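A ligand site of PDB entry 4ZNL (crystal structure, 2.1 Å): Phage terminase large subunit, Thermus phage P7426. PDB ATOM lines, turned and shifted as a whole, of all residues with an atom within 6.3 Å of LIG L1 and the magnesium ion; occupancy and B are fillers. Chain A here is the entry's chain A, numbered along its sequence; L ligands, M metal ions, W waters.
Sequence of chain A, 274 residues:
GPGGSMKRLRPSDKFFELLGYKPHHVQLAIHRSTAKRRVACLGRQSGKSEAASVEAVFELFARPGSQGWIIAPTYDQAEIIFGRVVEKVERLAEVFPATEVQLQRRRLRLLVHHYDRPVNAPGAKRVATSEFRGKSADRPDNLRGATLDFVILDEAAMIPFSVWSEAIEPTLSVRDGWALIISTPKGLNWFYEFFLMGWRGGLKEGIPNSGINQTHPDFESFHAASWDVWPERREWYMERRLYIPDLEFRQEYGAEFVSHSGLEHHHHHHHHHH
The side-chain carboxylate of Asp 154 lies close to the side-chain hydroxyl of Ser 49 (2.6 Å). NH2 of Arg 84 lies within salt-bridge range of OE1 of Glu 50 (2.7 Å). NZ of Lys 48 is in salt-bridge range of OE2 of Glu 155 (3.4 Å). The side-chain amino group (NZ) of Lys 48 sits at hydrogen-bond distance from the backbone carbonyl oxygen (O) of Gly 43 (3.3 Å). OG1 of Thr 184 sits at hydrogen-bond distance from NZ of Lys 48, at 3.4 Å. The backbone NH (N) of His 24 sits at hydrogen-bond distance from the side-chain amide oxygen (OE1) of Gln 27 (3.0 Å). The side-chain amide oxygen of Gln 27 lies close to the side-chain hydroxyl of Tyr 21, at 3.4 Å. OG1 of Thr 184 is in hydrogen-bond range of N of Arg 44, at 3.4 Å.
Water W3 lies within hydrogen-bond range of an oxygen (O4) of LIG L1 and the guanidinium group (NH1) of Arg 84. Water W5 bridges the backbone NH (N) of Lys 22 (2.8 Å) and a nitrogen (N4) of LIG L1 (2.9 Å).
N of Ser 49 lies within hydrogen-bond range of O5 of LIG L1, 3.1 Å away. The guanidinium group (NH1) of Arg 84 lies within salt-bridge range of an oxygen (O4) of LIG L1, 2.7 Å away. O2 of LIG L1 is in hydrogen-bond range of N of Lys 48. NZ of Lys 48 lies within salt-bridge range of O2 of LIG L1 (3.2 Å). The backbone NH of Gln 45 lies close to an oxygen (O1) of LIG L1, at 2.7 Å. The backbone NH (N) of Gly 47 is in hydrogen-bond range of an oxygen (O2) of LIG L1. The backbone carbonyl oxygen (O) of Lys 22 is in hydrogen-bond range of a nitrogen (N3) of LIG L1. The backbone NH (N) of Glu 50 is in hydrogen-bond range of an oxygen (O5) of LIG L1, 2.8 Å away. The side-chain amide oxygen (OE1) of Gln 27 is in hydrogen-bond range of a nitrogen (N3) of LIG L1 (2.8 Å). The backbone NH of Ser 46 sits at hydrogen-bond distance from an oxygen (O2) of LIG L1. F1 of LG2 L2 sits at hydrogen-bond distance from NZ of Lys 48, at 3.4 Å. The side-chain amide oxygen (OE1) of Gln 45 lies close to a fluorine (F2) of LG2 L2, 3.0 Å away.
Tyr 21 touches LIG L1. CA of Pro 23 touches N3 of LIG L1 (3.7 Å). His 24 touches LIG L1 (NE2 to N3, 3.5 Å). Arg 44 touches LIG L1. CH2 of Trp 230 touches O8 of LIG L1 (3.2 Å). Of the 21 residues printed, 14 come within 4 Å of LIG L1. The nearest printed residue that does not touch LIG L1 is Gly 43 (4.2 Å).
The magnesium ion is bound by F3 of LG2 L2. The magnesium ion is bound by OG of Ser 49 (2.0 Å). Water W3 binds the magnesium ion, 2.0 Å away. O3 of LIG L1 binds the magnesium ion, 2.1 Å away. Water W4 is bound to the magnesium ion. Water W2 is bound to the magnesium ion (2.3 Å). The magnesium ion has six donor atoms within binding distance.
BE1 of LG2 L2 is bound by O1 of LIG L1 (1.7 Å).
OD2 of Asp 154 touches the magnesium ion, 3.95 Å away. Within 4 Å of the magnesium ion: Ser 49 and Asp 154. Along chain A the residues within 4 Å of the magnesium ion span positions 49 to 154.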
ATOM      1  N   TYR A  21      34.553 -10.926 -21.082  1.00  0.00           N
ATOM      2  CA  TYR A  21      33.529 -11.724 -20.415  1.00  0.00           C
ATOM      3  C   TYR A  21      33.216 -11.130 -19.040  1.00  0.00           C
ATOM      4  O   TYR A  21      34.106 -10.961 -18.222  1.00  0.00           O
ATOM      5  CB  TYR A  21      34.019 -13.167 -20.292  1.00  0.00           C
ATOM      6  CG  TYR A  21      33.196 -14.115 -19.448  1.00  0.00           C
ATOM      7  CD1 TYR A  21      31.896 -14.477 -19.807  1.00  0.00           C
ATOM      8  CD2 TYR A  21      33.745 -14.716 -18.320  1.00  0.00           C
ATOM      9  CE1 TYR A  21      31.166 -15.386 -19.037  1.00  0.00           C
ATOM     10  CE2 TYR A  21      33.033 -15.606 -17.561  1.00  0.00           C
ATOM     11  CZ  TYR A  21      31.748 -15.937 -17.915  1.00  0.00           C
ATOM     12  OH  TYR A  21      31.069 -16.852 -17.142  1.00  0.00           O
ATOM     13  N   LYS A  22      31.949 -10.797 -18.828  1.00  0.00           N
ATOM     14  CA  LYS A  22      31.484 -10.278 -17.545  1.00  0.00           C
ATOM     15  C   LYS A  22      30.526 -11.279 -16.896  1.00  0.00           C
ATOM     16  O   LYS A  22      29.324 -11.237 -17.164  1.00  0.00           O
ATOM     17  CB  LYS A  22      30.790  -8.922 -17.723  1.00  0.00           C
ATOM     18  CG  LYS A  22      31.716  -7.726 -17.743  1.00  0.00           C
ATOM     19  CD  LYS A  22      31.969  -7.194 -19.152  1.00  0.00           C
ATOM     20  CE  LYS A  22      32.525  -5.775 -19.096  1.00  0.00           C
ATOM     21  NZ  LYS A  22      32.647  -5.155 -20.449  1.00  0.00           N
ATOM     22  N   PRO A  23      31.062 -12.183 -16.063  1.00  0.00           N
ATOM     23  CA  PRO A  23      30.185 -13.206 -15.482  1.00  0.00           C
ATOM     24  C   PRO A  23      29.127 -12.670 -14.515  1.00  0.00           C
ATOM     25  O   PRO A  23      29.412 -11.774 -13.721  1.00  0.00           O
ATOM     26  CB  PRO A  23      31.170 -14.122 -14.743  1.00  0.00           C
ATOM     27  CG  PRO A  23      32.382 -13.310 -14.551  1.00  0.00           C
ATOM     28  CD  PRO A  23      32.465 -12.388 -15.699  1.00  0.00           C
ATOM     29  N   HIS A  24      27.915 -13.243 -14.585  1.00  0.00           N
ATOM     30  CA  HIS A  24      26.873 -13.019 -13.575  1.00  0.00           C
ATOM     31  C   HIS A  24      27.379 -13.540 -12.248  1.00  0.00           C
ATOM     32  O   HIS A  24      28.351 -14.277 -12.210  1.00  0.00           O
ATOM     33  CB  HIS A  24      25.572 -13.750 -13.929  1.00  0.00           C
ATOM     34  CG  HIS A  24      25.099 -13.512 -15.323  1.00  0.00           C
ATOM     35  ND1 HIS A  24      24.736 -12.262 -15.795  1.00  0.00           N
ATOM     36  CD2 HIS A  24      24.892 -14.370 -16.349  1.00  0.00           C
ATOM     37  CE1 HIS A  24      24.338 -12.372 -17.053  1.00  0.00           C
ATOM     38  NE2 HIS A  24      24.420 -13.647 -17.414  1.00  0.00           N
ATOM     39  N   GLN A  27      27.642 -17.330 -12.216  1.00  0.00           N
ATOM     40  CA  GLN A  27      28.796 -17.762 -12.985  1.00  0.00           C
ATOM     41  C   GLN A  27      30.091 -17.553 -12.209  1.00  0.00           C
ATOM     42  O   GLN A  27      30.952 -18.426 -12.153  1.00  0.00           O
ATOM     43  CB  GLN A  27      28.865 -17.016 -14.319  1.00  0.00           C
ATOM     44  CG  GLN A  27      27.918 -17.569 -15.366  1.00  0.00           C
ATOM     45  CD  GLN A  27      27.811 -16.686 -16.590  1.00  0.00           C
ATOM     46  OE1 GLN A  27      28.002 -15.476 -16.517  1.00  0.00           O
ATOM     47  NE2 GLN A  27      27.514 -17.295 -17.729  1.00  0.00           N
ATOM     48  N   LEU A  42      21.000 -24.797 -13.585  1.00  0.00           N
ATOM     49  CA  LEU A  42      20.607 -23.457 -14.006  1.00  0.00           C
ATOM     50  C   LEU A  42      19.526 -23.481 -15.086  1.00  0.00           C
ATOM     51  O   LEU A  42      19.421 -24.427 -15.864  1.00  0.00           O
ATOM     52  CB  LEU A  42      21.824 -22.676 -14.539  1.00  0.00           C
ATOM     53  CG  LEU A  42      23.122 -22.751 -13.732  1.00  0.00           C
ATOM     54  CD1 LEU A  42      24.246 -21.991 -14.425  1.00  0.00           C
ATOM     55  CD2 LEU A  42      22.920 -22.226 -12.342  1.00  0.00           C
ATOM     56  N   GLY A  43      18.733 -22.418 -15.120  1.00  0.00           N
ATOM     57  CA  GLY A  43      17.675 -22.276 -16.093  1.00  0.00           C
ATOM     58  C   GLY A  43      18.160 -22.026 -17.511  1.00  0.00           C
ATOM     59  O   GLY A  43      19.315 -21.622 -17.723  1.00  0.00           O
ATOM     60  N   ARG A  44      17.279 -22.287 -18.476  1.00  0.00           N
ATOM     61  CA  ARG A  44      17.497 -21.969 -19.892  1.00  0.00           C
ATOM     62  C   ARG A  44      18.040 -20.560 -20.103  1.00  0.00           C
ATOM     63  O   ARG A  44      17.598 -19.616 -19.460  1.00  0.00           O
ATOM     64  CB  ARG A  44      16.187 -22.070 -20.692  1.00  0.00           C
ATOM     65  CG  ARG A  44      15.808 -23.433 -21.192  1.00  0.00           C
ATOM     66  CD  ARG A  44      14.681 -23.333 -22.225  1.00  0.00           C
ATOM     67  NE  ARG A  44      15.199 -23.192 -23.589  1.00  0.00           N
ATOM     68  CZ  ARG A  44      15.349 -22.041 -24.254  1.00  0.00           C
ATOM     69  NH1 ARG A  44      15.013 -20.881 -23.706  1.00  0.00           N
ATOM     70  NH2 ARG A  44      15.840 -22.064 -25.483  1.00  0.00           N
ATOM     71  N   GLN A  45      18.997 -20.448 -21.021  1.00  0.00           N
ATOM     72  CA  GLN A  45      19.560 -19.165 -21.438  1.00  0.00           C
ATOM     73  C   GLN A  45      20.196 -18.389 -20.289  1.00  0.00           C
ATOM     74  O   GLN A  45      20.273 -17.166 -20.329  1.00  0.00           O
ATOM     75  CB  GLN A  45      18.477 -18.308 -22.113  1.00  0.00           C
ATOM     76  CG  GLN A  45      18.075 -18.833 -23.472  1.00  0.00           C
ATOM     77  CD  GLN A  45      19.164 -18.649 -24.508  1.00  0.00           C
ATOM     78  OE1 GLN A  45      19.663 -19.604 -25.090  1.00  0.00           O
ATOM     79  NE2 GLN A  45      19.551 -17.403 -24.728  1.00  0.00           N
ATOM     80  N   SER A  46      20.692 -19.102 -19.278  1.00  0.00           N
ATOM     81  CA  SER A  46      21.308 -18.461 -18.118  1.00  0.00           C
ATOM     82  C   SER A  46      22.815 -18.220 -18.314  1.00  0.00           C
ATOM     83  O   SER A  46      23.428 -17.425 -17.585  1.00  0.00           O
ATOM     84  CB  SER A  46      21.072 -19.313 -16.867  1.00  0.00           C
ATOM     85  OG  SER A  46      21.532 -20.633 -17.067  1.00  0.00           O
ATOM     86  N   GLY A  47      23.402 -18.917 -19.287  1.00  0.00           N
ATOM     87  CA  GLY A  47      24.827 -18.837 -19.531  1.00  0.00           C
ATOM     88  C   GLY A  47      25.576 -20.098 -19.130  1.00  0.00           C
ATOM     89  O   GLY A  47      26.751 -20.050 -18.733  1.00  0.00           O
ATOM     90  N   LYS A  48      24.907 -21.244 -19.219  1.00  0.00           N
ATOM     91  CA  LYS A  48      25.547 -22.520 -18.936  1.00  0.00           C
ATOM     92  C   LYS A  48      26.634 -22.820 -19.966  1.00  0.00           C
ATOM     93  O   LYS A  48      27.771 -23.135 -19.615  1.00  0.00           O
ATOM     94  CB  LYS A  48      24.517 -23.641 -18.908  1.00  0.00           C
ATOM     95  CG  LYS A  48      23.474 -23.455 -17.817  1.00  0.00           C
ATOM     96  CD  LYS A  48      22.556 -24.658 -17.647  1.00  0.00           C
ATOM     97  CE  LYS A  48      21.825 -24.977 -18.906  1.00  0.00           C
ATOM     98  NZ  LYS A  48      21.009 -23.860 -19.415  1.00  0.00           N
ATOM     99  N   SER A  49      26.284 -22.725 -21.232  1.00  0.00           N
ATOM    100  CA  SER A  49      27.225 -23.056 -22.284  1.00  0.00           C
ATOM    101  C   SER A  49      28.331 -22.022 -22.316  1.00  0.00           C
ATOM    102  O   SER A  49      29.480 -22.340 -22.593  1.00  0.00           O
ATOM    103  CB  SER A  49      26.506 -23.147 -23.629  1.00  0.00           C
ATOM    104  OG  SER A  49      25.642 -24.263 -23.644  1.00  0.00           O
ATOM    105  N   GLU A  50      27.984 -20.773 -22.008  1.00  0.00           N
ATOM    106  CA  GLU A  50      28.966 -19.711 -21.962  1.00  0.00           C
ATOM    107  C   GLU A  50      30.011 -20.018 -20.888  1.00  0.00           C
ATOM    108  O   GLU A  50      31.223 -19.938 -21.141  1.00  0.00           O
ATOM    109  CB  GLU A  50      28.291 -18.362 -21.703  1.00  0.00           C
ATOM    110  CG  GLU A  50      29.233 -17.172 -21.780  1.00  0.00           C
ATOM    111  CD  GLU A  50      29.680 -16.871 -23.209  1.00  0.00           C
ATOM    112  OE1 GLU A  50      29.063 -17.383 -24.162  1.00  0.00           O
ATOM    113  OE2 GLU A  50      30.650 -16.115 -23.365  1.00  0.00           O
ATOM    114  N   ALA A  51      29.552 -20.354 -19.693  1.00  0.00           N
ATOM    115  CA  ALA A  51      30.451 -20.653 -18.594  1.00  0.00           C
ATOM    116  C   ALA A  51      31.323 -21.867 -18.914  1.00  0.00           C
ATOM    117  O   ALA A  51      32.518 -21.911 -18.569  1.00  0.00           O
ATOM    118  CB  ALA A  51      29.651 -20.893 -17.307  1.00  0.00           C
ATOM    119  N   ILE A  81      29.197 -25.759 -29.481  1.00  0.00           N
ATOM    120  CA  ILE A  81      29.970 -25.237 -28.373  1.00  0.00           C
ATOM    121  C   ILE A  81      31.468 -25.285 -28.719  1.00  0.00           C
ATOM    122  O   ILE A  81      32.220 -24.429 -28.265  1.00  0.00           O
ATOM    123  CB  ILE A  81      29.679 -25.991 -27.043  1.00  0.00           C
ATOM    124  CG1 ILE A  81      30.157 -25.138 -25.861  1.00  0.00           C
ATOM    125  CG2 ILE A  81      30.321 -27.360 -27.035  1.00  0.00           C
ATOM    126  CD1 ILE A  81      29.528 -25.503 -24.539  1.00  0.00           C
ATOM    127  N   ARG A  84      32.127 -22.085 -30.313  1.00  0.00           N
ATOM    128  CA  ARG A  84      32.147 -20.986 -29.352  1.00  0.00           C
ATOM    129  C   ARG A  84      33.468 -20.921 -28.598  1.00  0.00           C
ATOM    130  O   ARG A  84      33.960 -19.821 -28.292  1.00  0.00           O
ATOM    131  CB  ARG A  84      30.981 -21.107 -28.357  1.00  0.00           C
ATOM    132  CG  ARG A  84      29.633 -20.731 -28.946  1.00  0.00           C
ATOM    133  CD  ARG A  84      28.472 -21.098 -28.016  1.00  0.00           C
ATOM    134  NE  ARG A  84      28.385 -20.195 -26.872  1.00  0.00           N
ATOM    135  CZ  ARG A  84      27.332 -20.088 -26.070  1.00  0.00           C
ATOM    136  NH1 ARG A  84      26.253 -20.831 -26.286  1.00  0.00           N
ATOM    137  NH2 ARG A  84      27.347 -19.233 -25.060  1.00  0.00           N
ATOM    138  N   ASP A 154      27.936 -30.446 -20.569  1.00  0.00           N
ATOM    139  CA  ASP A 154      26.920 -29.424 -20.854  1.00  0.00           C
ATOM    140  C   ASP A 154      25.573 -30.131 -21.094  1.00  0.00           C
ATOM    141  O   ASP A 154      25.523 -31.175 -21.744  1.00  0.00           O
ATOM    142  CB  ASP A 154      27.357 -28.578 -22.055  1.00  0.00           C
ATOM    143  CG  ASP A 154      26.585 -27.277 -22.181  1.00  0.00           C
ATOM    144  OD1 ASP A 154      25.844 -26.923 -21.232  1.00  0.00           O
ATOM    145  OD2 ASP A 154      26.727 -26.595 -23.217  1.00  0.00           O
ATOM    146  N   GLU A 155      24.501 -29.560 -20.560  1.00  0.00           N
ATOM    147  CA  GLU A 155      23.192 -30.219 -20.441  1.00  0.00           C
ATOM    148  C   GLU A 155      23.318 -31.650 -19.945  1.00  0.00           C
ATOM    149  O   GLU A 155      22.779 -32.614 -20.524  1.00  0.00           O
ATOM    150  CB  GLU A 155      22.442 -30.188 -21.774  1.00  0.00           C
ATOM    151  CG  GLU A 155      22.073 -28.781 -22.242  1.00  0.00           C
ATOM    152  CD  GLU A 155      21.437 -27.919 -21.138  1.00  0.00           C
ATOM    153  OE1 GLU A 155      20.695 -28.435 -20.280  1.00  0.00           O
ATOM    154  OE2 GLU A 155      21.706 -26.702 -21.143  1.00  0.00           O
ATOM    155  N   THR A 184      20.192 -27.649 -17.289  1.00  0.00           N
ATOM    156  CA  THR A 184      18.819 -27.479 -16.869  1.00  0.00           C
ATOM    157  C   THR A 184      18.353 -28.870 -16.422  1.00  0.00           C
ATOM    158  O   THR A 184      18.670 -29.858 -17.072  1.00  0.00           O
ATOM    159  CB  THR A 184      17.951 -26.903 -18.011  1.00  0.00           C
ATOM    160  OG1 THR A 184      18.318 -25.539 -18.226  1.00  0.00           O
ATOM    161  CG2 THR A 184      16.452 -26.961 -17.685  1.00  0.00           C
ATOM    162  N   TRP A 230      19.955 -13.675 -14.087  1.00  0.00           N
ATOM    163  CA  TRP A 230      19.810 -12.517 -14.967  1.00  0.00           C
ATOM    164  C   TRP A 230      18.578 -11.708 -14.552  1.00  0.00           C
ATOM    165  O   TRP A 230      17.599 -11.628 -15.291  1.00  0.00           O
ATOM    166  CB  TRP A 230      19.717 -12.999 -16.432  1.00  0.00           C
ATOM    167  CG  TRP A 230      20.598 -12.274 -17.398  1.00  0.00           C
ATOM    168  CD1 TRP A 230      21.091 -11.002 -17.279  1.00  0.00           C
ATOM    169  CD2 TRP A 230      21.109 -12.782 -18.640  1.00  0.00           C
ATOM    170  NE1 TRP A 230      21.859 -10.687 -18.374  1.00  0.00           N
ATOM    171  CE2 TRP A 230      21.884 -11.761 -19.229  1.00  0.00           C
ATOM    172  CE3 TRP A 230      20.968 -13.998 -19.318  1.00  0.00           C
ATOM    173  CZ2 TRP A 230      22.517 -11.911 -20.454  1.00  0.00           C
ATOM    174  CZ3 TRP A 230      21.610 -14.146 -20.542  1.00  0.00           C
ATOM    175  CH2 TRP A 230      22.372 -13.116 -21.103  1.00  0.00           C
HETATM  176  P1  LIG L   1      22.447 -21.492 -21.963  1.00  0.00           P
HETATM  177  O1  LIG L   1      20.955 -21.901 -22.264  1.00  0.00           O
HETATM  178  O2  LIG L   1      22.490 -21.208 -20.482  1.00  0.00           O
HETATM  179  O3  LIG L   1      23.481 -22.550 -22.330  1.00  0.00           O
HETATM  180  P2  LIG L   1      24.066 -19.646 -23.294  1.00  0.00           P
HETATM  181  O4  LIG L   1      24.205 -20.051 -24.767  1.00  0.00           O
HETATM  182  O5  LIG L   1      25.306 -20.080 -22.542  1.00  0.00           O
HETATM  183  O6  LIG L   1      22.708 -20.193 -22.758  1.00  0.00           O
HETATM  184  O7  LIG L   1      23.921 -18.106 -23.157  1.00  0.00           O
HETATM  185  C1  LIG L   1      22.848 -17.489 -23.731  1.00  0.00           C
HETATM  186  C2  LIG L   1      23.085 -16.118 -24.292  1.00  0.00           C
HETATM  187  O8  LIG L   1      23.460 -15.255 -23.231  1.00  0.00           O
HETATM  188  C3  LIG L   1      24.199 -16.150 -25.216  1.00  0.00           C
HETATM  189  O9  LIG L   1      24.017 -15.235 -26.249  1.00  0.00           O
HETATM  190  C4  LIG L   1      25.349 -15.769 -24.402  1.00  0.00           C
HETATM  191  O10 LIG L   1      26.311 -15.141 -25.194  1.00  0.00           O
HETATM  192  C5  LIG L   1      24.796 -14.834 -23.440  1.00  0.00           C
HETATM  193  N1  LIG L   1      25.466 -14.829 -22.180  1.00  0.00           N
HETATM  194  C6  LIG L   1      25.630 -15.844 -21.317  1.00  0.00           C
HETATM  195  N2  LIG L   1      26.302 -15.363 -20.250  1.00  0.00           N
HETATM  196  C7  LIG L   1      26.559 -14.030 -20.428  1.00  0.00           C
HETATM  197  C8  LIG L   1      27.213 -13.016 -19.656  1.00  0.00           C
HETATM  198  N3  LIG L   1      27.824 -13.317 -18.322  1.00  0.00           N
HETATM  199  N4  LIG L   1      27.291 -11.773 -20.151  1.00  0.00           N
HETATM  200  C9  LIG L   1      26.759 -11.471 -21.363  1.00  0.00           C
HETATM  201  N5  LIG L   1      26.139 -12.395 -22.108  1.00  0.00           N
HETATM  202  C10 LIG L   1      26.022 -13.682 -21.664  1.00  0.00           C
HETATM  203 BE1  LG2 L   2      20.490 -23.213 -23.314  1.00  0.00          BE
HETATM  204  F1  LG2 L   2      19.618 -24.152 -22.502  1.00  0.00           F
HETATM  205  F2  LG2 L   2      19.608 -22.534 -24.502  1.00  0.00           F
HETATM  206  F3  LG2 L   2      21.767 -24.008 -23.795  1.00  0.00           F
HETATM  207 MG    MG M   1      23.651 -24.154 -23.665  1.00  0.00          MG
HETATM  208  O   HOH W   1      24.687 -12.613 -27.619  1.00  0.00           O
HETATM  209  O   HOH W   2      23.239 -25.818 -25.189  1.00  0.00           O
HETATM  210  O   HOH W   3      23.663 -22.909 -25.251  1.00  0.00           O
HETATM  211  O   HOH W   4      23.567 -25.522 -22.064  1.00  0.00           O
HETATM  212  O   HOH W   5      29.997 -11.092 -20.758  1.00  0.00           O
